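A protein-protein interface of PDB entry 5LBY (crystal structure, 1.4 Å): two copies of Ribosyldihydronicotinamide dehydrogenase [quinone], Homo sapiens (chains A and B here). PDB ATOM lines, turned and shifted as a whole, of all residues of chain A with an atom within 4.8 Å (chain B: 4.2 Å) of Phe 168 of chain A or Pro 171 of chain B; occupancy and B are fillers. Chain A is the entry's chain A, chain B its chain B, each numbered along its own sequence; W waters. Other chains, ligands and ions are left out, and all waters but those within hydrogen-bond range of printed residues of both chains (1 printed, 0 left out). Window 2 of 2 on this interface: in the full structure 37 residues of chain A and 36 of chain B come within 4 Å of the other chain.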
ATOM      1  N   LEU A 104      11.856 -11.909  -6.536  1.00  0.00           N
ATOM      2  CA  LEU A 104      11.661 -13.242  -7.073  1.00  0.00           C
ATOM      3  C   LEU A 104      11.143 -14.140  -5.966  1.00  0.00           C
ATOM      4  O   LEU A 104      11.752 -14.201  -4.882  1.00  0.00           O
ATOM      5  CB  LEU A 104      12.996 -13.746  -7.610  1.00  0.00           C
ATOM      6  CG  LEU A 104      12.991 -14.969  -8.521  1.00  0.00           C
ATOM      7  CD1 LEU A 104      12.258 -14.718  -9.819  1.00  0.00           C
ATOM      8  CD2 LEU A 104      14.397 -15.446  -8.789  1.00  0.00           C
ATOM      9  N   TRP A 106      10.116 -18.163  -5.607  1.00  0.00           N
ATOM     10  CA  TRP A 106      10.078 -19.482  -6.268  1.00  0.00           C
ATOM     11  C   TRP A 106      10.259 -19.339  -7.770  1.00  0.00           C
ATOM     12  O   TRP A 106       9.552 -19.919  -8.589  1.00  0.00           O
ATOM     13  CB  TRP A 106       8.780 -20.250  -5.927  1.00  0.00           C
ATOM     14  CG  TRP A 106       8.765 -20.742  -4.541  1.00  0.00           C
ATOM     15  CD1 TRP A 106       7.841 -20.470  -3.587  1.00  0.00           C
ATOM     16  CD2 TRP A 106       9.684 -21.678  -3.957  1.00  0.00           C
ATOM     17  NE1 TRP A 106       8.136 -21.157  -2.428  1.00  0.00           N
ATOM     18  CE2 TRP A 106       9.291 -21.885  -2.615  1.00  0.00           C
ATOM     19  CE3 TRP A 106      10.810 -22.349  -4.420  1.00  0.00           C
ATOM     20  CZ2 TRP A 106       9.970 -22.759  -1.777  1.00  0.00           C
ATOM     21  CZ3 TRP A 106      11.519 -23.163  -3.568  1.00  0.00           C
ATOM     22  CH2 TRP A 106      11.089 -23.343  -2.268  1.00  0.00           C
ATOM     23  N   PHE A 107      11.298 -18.566  -8.139  1.00  0.00           N
ATOM     24  CA  PHE A 107      11.719 -18.476  -9.534  1.00  0.00           C
ATOM     25  C   PHE A 107      10.592 -17.955 -10.413  1.00  0.00           C
ATOM     26  O   PHE A 107      10.562 -18.235 -11.623  1.00  0.00           O
ATOM     27  CB  PHE A 107      12.317 -19.779 -10.044  1.00  0.00           C
ATOM     28  CG  PHE A 107      13.491 -20.213  -9.143  1.00  0.00           C
ATOM     29  CD1 PHE A 107      14.742 -19.589  -9.249  1.00  0.00           C
ATOM     30  CD2 PHE A 107      13.320 -21.088  -8.103  1.00  0.00           C
ATOM     31  CE1 PHE A 107      15.780 -19.938  -8.431  1.00  0.00           C
ATOM     32  CE2 PHE A 107      14.392 -21.430  -7.268  1.00  0.00           C
ATOM     33  CZ  PHE A 107      15.596 -20.850  -7.437  1.00  0.00           C
ATOM     34  N   TYR A 156      23.206 -17.543 -10.612  1.00  0.00           N
ATOM     35  CA  TYR A 156      22.308 -17.411 -11.741  1.00  0.00           C
ATOM     36  C   TYR A 156      22.978 -17.472 -13.080  1.00  0.00           C
ATOM     37  O   TYR A 156      22.452 -16.976 -14.096  1.00  0.00           O
ATOM     38  CB  TYR A 156      21.429 -16.184 -11.576  1.00  0.00           C
ATOM     39  CG  TYR A 156      20.328 -16.401 -10.563  1.00  0.00           C
ATOM     40  CD1 TYR A 156      19.298 -17.270 -10.814  1.00  0.00           C
ATOM     41  CD2 TYR A 156      20.364 -15.730  -9.319  1.00  0.00           C
ATOM     42  CE1 TYR A 156      18.341 -17.527  -9.864  1.00  0.00           C
ATOM     43  CE2 TYR A 156      19.362 -15.947  -8.376  1.00  0.00           C
ATOM     44  CZ  TYR A 156      18.332 -16.805  -8.689  1.00  0.00           C
ATOM     45  OH  TYR A 156      17.344 -17.039  -7.778  1.00  0.00           O
ATOM     46  N   ASP A 164      20.848 -20.657 -15.257  1.00  0.00           N
ATOM     47  CA  ASP A 164      20.804 -19.332 -15.888  1.00  0.00           C
ATOM     48  C   ASP A 164      19.483 -18.637 -15.492  1.00  0.00           C
ATOM     49  O   ASP A 164      18.400 -19.214 -15.611  1.00  0.00           O
ATOM     50  CB  ASP A 164      20.851 -19.499 -17.419  1.00  0.00           C
ATOM     51  CG  ASP A 164      21.110 -18.259 -18.244  1.00  0.00           C
ATOM     52  OD1 ASP A 164      20.755 -17.172 -17.920  1.00  0.00           O
ATOM     53  OD2 ASP A 164      21.700 -18.462 -19.351  1.00  0.00           O
ATOM     54  N   SER A 165      19.604 -17.357 -15.145  1.00  0.00           N
ATOM     55  CA  SER A 165      18.405 -16.593 -14.871  1.00  0.00           C
ATOM     56  C   SER A 165      17.401 -16.573 -16.017  1.00  0.00           C
ATOM     57  O   SER A 165      16.164 -16.571 -15.803  1.00  0.00           O
ATOM     58  CB  SER A 165      18.721 -15.184 -14.454  1.00  0.00           C
ATOM     59  OG  SER A 165      19.503 -14.541 -15.411  1.00  0.00           O
ATOM     60  N   ARG A 166      17.923 -16.610 -17.241  1.00  0.00           N
ATOM     61  CA  ARG A 166      16.990 -16.582 -18.381  1.00  0.00           C
ATOM     62  C   ARG A 166      16.020 -17.761 -18.391  1.00  0.00           C
ATOM     63  O   ARG A 166      14.907 -17.661 -18.906  1.00  0.00           O
ATOM     64  CB  ARG A 166      17.767 -16.557 -19.716  1.00  0.00           C
ATOM     65  CG  ARG A 166      18.596 -15.319 -19.933  1.00  0.00           C
ATOM     66  CD  ARG A 166      19.118 -15.269 -21.339  1.00  0.00           C
ATOM     67  NE  ARG A 166      19.930 -14.073 -21.579  1.00  0.00           N
ATOM     68  CZ  ARG A 166      20.401 -13.717 -22.769  1.00  0.00           C
ATOM     69  NH1 ARG A 166      20.129 -14.427 -23.829  1.00  0.00           N
ATOM     70  NH2 ARG A 166      21.126 -12.633 -22.897  1.00  0.00           N
ATOM     71  N   TYR A 167      16.436 -18.884 -17.809  1.00  0.00           N
ATOM     72  CA  TYR A 167      15.613 -20.057 -17.866  1.00  0.00           C
ATOM     73  C   TYR A 167      14.260 -19.855 -17.262  1.00  0.00           C
ATOM     74  O   TYR A 167      13.271 -20.352 -17.818  1.00  0.00           O
ATOM     75  CB  TYR A 167      16.288 -21.232 -17.162  1.00  0.00           C
ATOM     76  CG  TYR A 167      17.555 -21.740 -17.759  1.00  0.00           C
ATOM     77  CD1 TYR A 167      17.898 -21.466 -19.081  1.00  0.00           C
ATOM     78  CD2 TYR A 167      18.399 -22.602 -17.040  1.00  0.00           C
ATOM     79  CE1 TYR A 167      19.063 -21.969 -19.648  1.00  0.00           C
ATOM     80  CE2 TYR A 167      19.522 -23.114 -17.603  1.00  0.00           C
ATOM     81  CZ  TYR A 167      19.852 -22.839 -18.932  1.00  0.00           C
ATOM     82  OH  TYR A 167      21.005 -23.334 -19.515  1.00  0.00           O
ATOM     83  N   PHE A 168      14.229 -19.275 -16.075  1.00  0.00           N
ATOM     84  CA  PHE A 168      12.946 -19.123 -15.438  1.00  0.00           C
ATOM     85  C   PHE A 168      12.200 -17.865 -15.841  1.00  0.00           C
ATOM     86  O   PHE A 168      11.059 -17.666 -15.496  1.00  0.00           O
ATOM     87  CB  PHE A 168      13.070 -19.265 -13.922  1.00  0.00           C
ATOM     88  CG  PHE A 168      14.009 -18.327 -13.329  1.00  0.00           C
ATOM     89  CD1 PHE A 168      13.674 -17.045 -13.095  1.00  0.00           C
ATOM     90  CD2 PHE A 168      15.321 -18.785 -12.963  1.00  0.00           C
ATOM     91  CE1 PHE A 168      14.587 -16.167 -12.531  1.00  0.00           C
ATOM     92  CE2 PHE A 168      16.202 -17.888 -12.436  1.00  0.00           C
ATOM     93  CZ  PHE A 168      15.825 -16.556 -12.217  1.00  0.00           C
ATOM     94  N   LEU A 169      12.810 -17.022 -16.665  1.00  0.00           N
ATOM     95  CA  LEU A 169      12.109 -15.874 -17.209  1.00  0.00           C
ATOM     96  C   LEU A 169      11.100 -16.246 -18.301  1.00  0.00           C
ATOM     97  O   LEU A 169      10.200 -15.461 -18.627  1.00  0.00           O
ATOM     98  CB  LEU A 169      13.087 -14.832 -17.753  1.00  0.00           C
ATOM     99  CG  LEU A 169      13.958 -14.128 -16.733  1.00  0.00           C
ATOM    100  CD1 LEU A 169      14.959 -13.243 -17.419  1.00  0.00           C
ATOM    101  CD2 LEU A 169      13.119 -13.345 -15.738  1.00  0.00           C
ATOM    102  N   TRP A 170      11.257 -17.442 -18.857  1.00  0.00           N
ATOM    103  CA  TRP A 170      10.416 -17.886 -20.001  1.00  0.00           C
ATOM    104  C   TRP A 170       8.892 -17.765 -19.789  1.00  0.00           C
ATOM    105  O   TRP A 170       8.225 -17.202 -20.633  1.00  0.00           O
ATOM    106  CB  TRP A 170      10.830 -19.285 -20.377  1.00  0.00           C
ATOM    107  CG  TRP A 170      10.016 -20.030 -21.347  1.00  0.00           C
ATOM    108  CD1 TRP A 170       9.144 -21.052 -21.121  1.00  0.00           C
ATOM    109  CD2 TRP A 170      10.046 -19.856 -22.781  1.00  0.00           C
ATOM    110  NE1 TRP A 170       8.625 -21.513 -22.303  1.00  0.00           N
ATOM    111  CE2 TRP A 170       9.160 -20.801 -23.357  1.00  0.00           C
ATOM    112  CE3 TRP A 170      10.699 -18.951 -23.639  1.00  0.00           C
ATOM    113  CZ2 TRP A 170       8.961 -20.911 -24.699  1.00  0.00           C
ATOM    114  CZ3 TRP A 170      10.509 -19.093 -25.004  1.00  0.00           C
ATOM    115  CH2 TRP A 170       9.666 -20.069 -25.518  1.00  0.00           C
ATOM    116  N   PRO A 171       8.347 -18.338 -18.677  1.00  0.00           N
ATOM    117  CA  PRO A 171       6.906 -18.222 -18.511  1.00  0.00           C
ATOM    118  C   PRO A 171       6.401 -16.788 -18.466  1.00  0.00           C
ATOM    119  O   PRO A 171       5.284 -16.517 -18.850  1.00  0.00           O
ATOM    120  CB  PRO A 171       6.627 -18.946 -17.179  1.00  0.00           C
ATOM    121  CG  PRO A 171       7.801 -19.815 -17.009  1.00  0.00           C
ATOM    122  CD  PRO A 171       8.978 -19.114 -17.607  1.00  0.00           C
ATOM    123  N   LEU A 172       7.218 -15.899 -17.899  1.00  0.00           N
ATOM    124  CA  LEU A 172       6.870 -14.502 -17.722  1.00  0.00           C
ATOM    125  C   LEU A 172       7.037 -13.721 -18.993  1.00  0.00           C
ATOM    126  O   LEU A 172       6.108 -13.119 -19.522  1.00  0.00           O
ATOM    127  CB  LEU A 172       7.663 -13.886 -16.567  1.00  0.00           C
ATOM    128  CG  LEU A 172       7.508 -14.552 -15.198  1.00  0.00           C
ATOM    129  CD1 LEU A 172       8.523 -13.945 -14.231  1.00  0.00           C
ATOM    130  CD2 LEU A 172       6.137 -14.390 -14.682  1.00  0.00           C
ATOM    131  N   PHE B 168       8.441 -24.801 -19.533  1.00  0.00           N
ATOM    132  CA  PHE B 168       7.694 -24.150 -18.470  1.00  0.00           C
ATOM    133  C   PHE B 168       7.763 -24.904 -17.153  1.00  0.00           C
ATOM    134  O   PHE B 168       7.517 -24.360 -16.077  1.00  0.00           O
ATOM    135  CB  PHE B 168       6.263 -23.799 -18.883  1.00  0.00           C
ATOM    136  CG  PHE B 168       5.270 -24.951 -19.024  1.00  0.00           C
ATOM    137  CD1 PHE B 168       4.845 -25.658 -17.931  1.00  0.00           C
ATOM    138  CD2 PHE B 168       4.771 -25.326 -20.281  1.00  0.00           C
ATOM    139  CE1 PHE B 168       3.943 -26.675 -18.057  1.00  0.00           C
ATOM    140  CE2 PHE B 168       3.864 -26.340 -20.417  1.00  0.00           C
ATOM    141  CZ  PHE B 168       3.472 -27.052 -19.274  1.00  0.00           C
ATOM    142  N   LEU B 169       8.122 -26.203 -17.222  1.00  0.00           N
ATOM    143  CA  LEU B 169       8.187 -26.987 -16.025  1.00  0.00           C
ATOM    144  C   LEU B 169       9.364 -26.615 -15.121  1.00  0.00           C
ATOM    145  O   LEU B 169       9.365 -26.945 -13.930  1.00  0.00           O
ATOM    146  CB  LEU B 169       8.223 -28.490 -16.365  1.00  0.00           C
ATOM    147  CG  LEU B 169       6.975 -29.061 -16.982  1.00  0.00           C
ATOM    148  CD1 LEU B 169       7.228 -30.477 -17.451  1.00  0.00           C
ATOM    149  CD2 LEU B 169       5.802 -29.056 -16.019  1.00  0.00           C
ATOM    150  N   TRP B 170      10.403 -25.974 -15.683  1.00  0.00           N
ATOM    151  CA  TRP B 170      11.629 -25.744 -14.915  1.00  0.00           C
ATOM    152  C   TRP B 170      11.450 -25.041 -13.556  1.00  0.00           C
ATOM    153  O   TRP B 170      11.918 -25.560 -12.545  1.00  0.00           O
ATOM    154  CB  TRP B 170      12.619 -24.955 -15.807  1.00  0.00           C
ATOM    155  CG  TRP B 170      13.877 -24.504 -15.185  1.00  0.00           C
ATOM    156  CD1 TRP B 170      14.228 -23.231 -14.885  1.00  0.00           C
ATOM    157  CD2 TRP B 170      15.035 -25.302 -14.881  1.00  0.00           C
ATOM    158  NE1 TRP B 170      15.541 -23.195 -14.401  1.00  0.00           N
ATOM    159  CE2 TRP B 170      16.023 -24.467 -14.398  1.00  0.00           C
ATOM    160  CE3 TRP B 170      15.312 -26.673 -14.946  1.00  0.00           C
ATOM    161  CZ2 TRP B 170      17.311 -24.940 -14.051  1.00  0.00           C
ATOM    162  CZ3 TRP B 170      16.582 -27.112 -14.596  1.00  0.00           C
ATOM    163  CH2 TRP B 170      17.549 -26.258 -14.161  1.00  0.00           C
ATOM    164  N   PRO B 171      10.774 -23.863 -13.511  1.00  0.00           N
ATOM    165  CA  PRO B 171      10.643 -23.221 -12.213  1.00  0.00           C
ATOM    166  C   PRO B 171       9.840 -24.032 -11.188  1.00  0.00           C
ATOM    167  O   PRO B 171       9.969 -23.805 -10.001  1.00  0.00           O
ATOM    168  CB  PRO B 171       9.993 -21.884 -12.518  1.00  0.00           C
ATOM    169  CG  PRO B 171       9.982 -21.763 -13.976  1.00  0.00           C
ATOM    170  CD  PRO B 171      10.239 -23.056 -14.600  1.00  0.00           C
ATOM    171  N   LEU B 172       8.934 -24.896 -11.660  1.00  0.00           N
ATOM    172  CA  LEU B 172       8.033 -25.681 -10.844  1.00  0.00           C
ATOM    173  C   LEU B 172       8.760 -26.954 -10.376  1.00  0.00           C
ATOM    174  O   LEU B 172       8.972 -27.178  -9.187  1.00  0.00           O
ATOM    175  CB  LEU B 172       6.752 -25.995 -11.604  1.00  0.00           C
ATOM    176  CG  LEU B 172       5.920 -24.802 -12.029  1.00  0.00           C
ATOM    177  CD1 LEU B 172       4.749 -25.252 -12.886  1.00  0.00           C
ATOM    178  CD2 LEU B 172       5.439 -23.996 -10.851  1.00  0.00           C
ATOM    179  N   GLN B 173       9.114 -27.811 -11.326  1.00  0.00           N
ATOM    180  CA  GLN B 173       9.778 -29.065 -10.991  1.00  0.00           C
ATOM    181  C   GLN B 173      11.136 -28.863 -10.344  1.00  0.00           C
ATOM    182  O   GLN B 173      11.458 -29.499  -9.334  1.00  0.00           O
ATOM    183  CB  GLN B 173       9.939 -29.964 -12.232  1.00  0.00           C
ATOM    184  CG  GLN B 173       8.612 -30.485 -12.742  1.00  0.00           C
ATOM    185  CD  GLN B 173       8.736 -31.482 -13.842  1.00  0.00           C
ATOM    186  OE1 GLN B 173       9.784 -31.463 -14.641  1.00  0.00           O
ATOM    187  NE2 GLN B 173       7.781 -32.284 -14.028  1.00  0.00           N
ATOM    188  N   GLY B 175      12.944 -25.552  -9.778  1.00  0.00           N
ATOM    189  CA  GLY B 175      13.081 -24.406  -8.891  1.00  0.00           C
ATOM    190  C   GLY B 175      12.288 -24.496  -7.613  1.00  0.00           C
ATOM    191  O   GLY B 175      12.639 -23.836  -6.627  1.00  0.00           O
ATOM    192  N   THR B 176      11.230 -25.282  -7.611  1.00  0.00           N
ATOM    193  CA  THR B 176      10.382 -25.400  -6.417  1.00  0.00           C
ATOM    194  C   THR B 176      10.559 -26.801  -5.820  1.00  0.00           C
ATOM    195  O   THR B 176      11.039 -26.951  -4.685  1.00  0.00           O
ATOM    196  CB  THR B 176       8.912 -25.048  -6.674  1.00  0.00           C
ATOM    197  OG1 THR B 176       8.861 -23.749  -7.306  1.00  0.00           O
ATOM    198  CG2 THR B 176       8.124 -24.984  -5.393  1.00  0.00           C
HETATM  199  O   HOH W   1      17.508 -21.179 -13.854  1.00  0.00           O
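Gly 175 of chain B touches Trp 106 of chain A.
CE3 of Trp 106 of chain A touches CA of Thr 176 of chain B (3.7 Å).
CB of Pro 171 of chain B touches O of Phe 107 of chain A (3.8 Å).
Gly 175 of chain B touches Phe 107 of chain A.
NE1 of Trp 170 of chain B touches CB of Tyr 167 of chain A, 3.5 Å away.
CB of Phe 168 of chain A touches CG of Pro 171 of chain B, at 3.97 Å.
O of Trp 170 of chain B lies within hydrogen-bond range of N of Gly 175 of chain B.
The backbone carbonyl oxygen (O) of Pro 171 of chain B is in hydrogen-bond range of the side-chain hydroxyl (OG1) of Thr 176 of chain B (2.9 Å).
Hydrophobic or aromatic side chains of chain B that line the printed part of chain A: Trp 170 and Pro 171.
Along chain B the printed residues that touch a printed residue of chain A span positions 170 to 176.
Of the 13 printed residues of chain A, 4 touch a printed residue of chain B.
Hydrophobic or aromatic side chains of chain A that line the printed part of chain B: Trp 106, Phe 107, Tyr 167 and Phe 168.
Along chain A the printed residues that touch a printed residue of chain B span positions 106 to 168.
Among the printed residues, no Asp or Glu carboxylate lies within 4 Å of a Lys or Arg side-chain nitrogen of the other chain.
Phe 168 of chain A touches Pro 171 of chain B, but with the chains exchanged Pro 171 of chain A does not touch Phe 168 of chain B (4.6 Å).
Positions printed for both chains: 168, 169, 170, 171 and 172.
Of the printed residues of chain B, Trp 106 of chain A touches Gly 175 (3.2 Å) and Thr 176 (3.7 Å).
Arg 166 of chain A touches none of the printed residues of chain B.
Phe 168 of chain A touches just one residue of chain B: Pro 171.
Leu 169 of chain B touches none of the printed residues of chain A.
Printed residues of chain A within 4 Å of Trp 170 of chain B: Tyr 167.
Of chain A, only Phe 107 (3.8 Å) and Phe 168 (3.97 Å) come within 4 Å of Pro 171 of chain B.
Of the printed residues of chain A, Gly 175 of chain B touches Trp 106 (3.2 Å) and Phe 107 (3.0 Å).
The nearest residue of chain B that does not touch Phe 168 of chain A is Trp 170 of chain B (4.1 Å).
The nearest residue of chain A that does not touch Pro 171 of chain B is Trp 106 of chain A (4.2 Å).
The nearest printed residue of chain B that does not touch Tyr 167 of chain A is Pro 171 of chain B (5.2 Å).
Water W1 lies within hydrogen-bond range of O of Asp 164 of chain A (2.8 Å) and NE1 of Trp 170 of chain B (2.9 Å).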
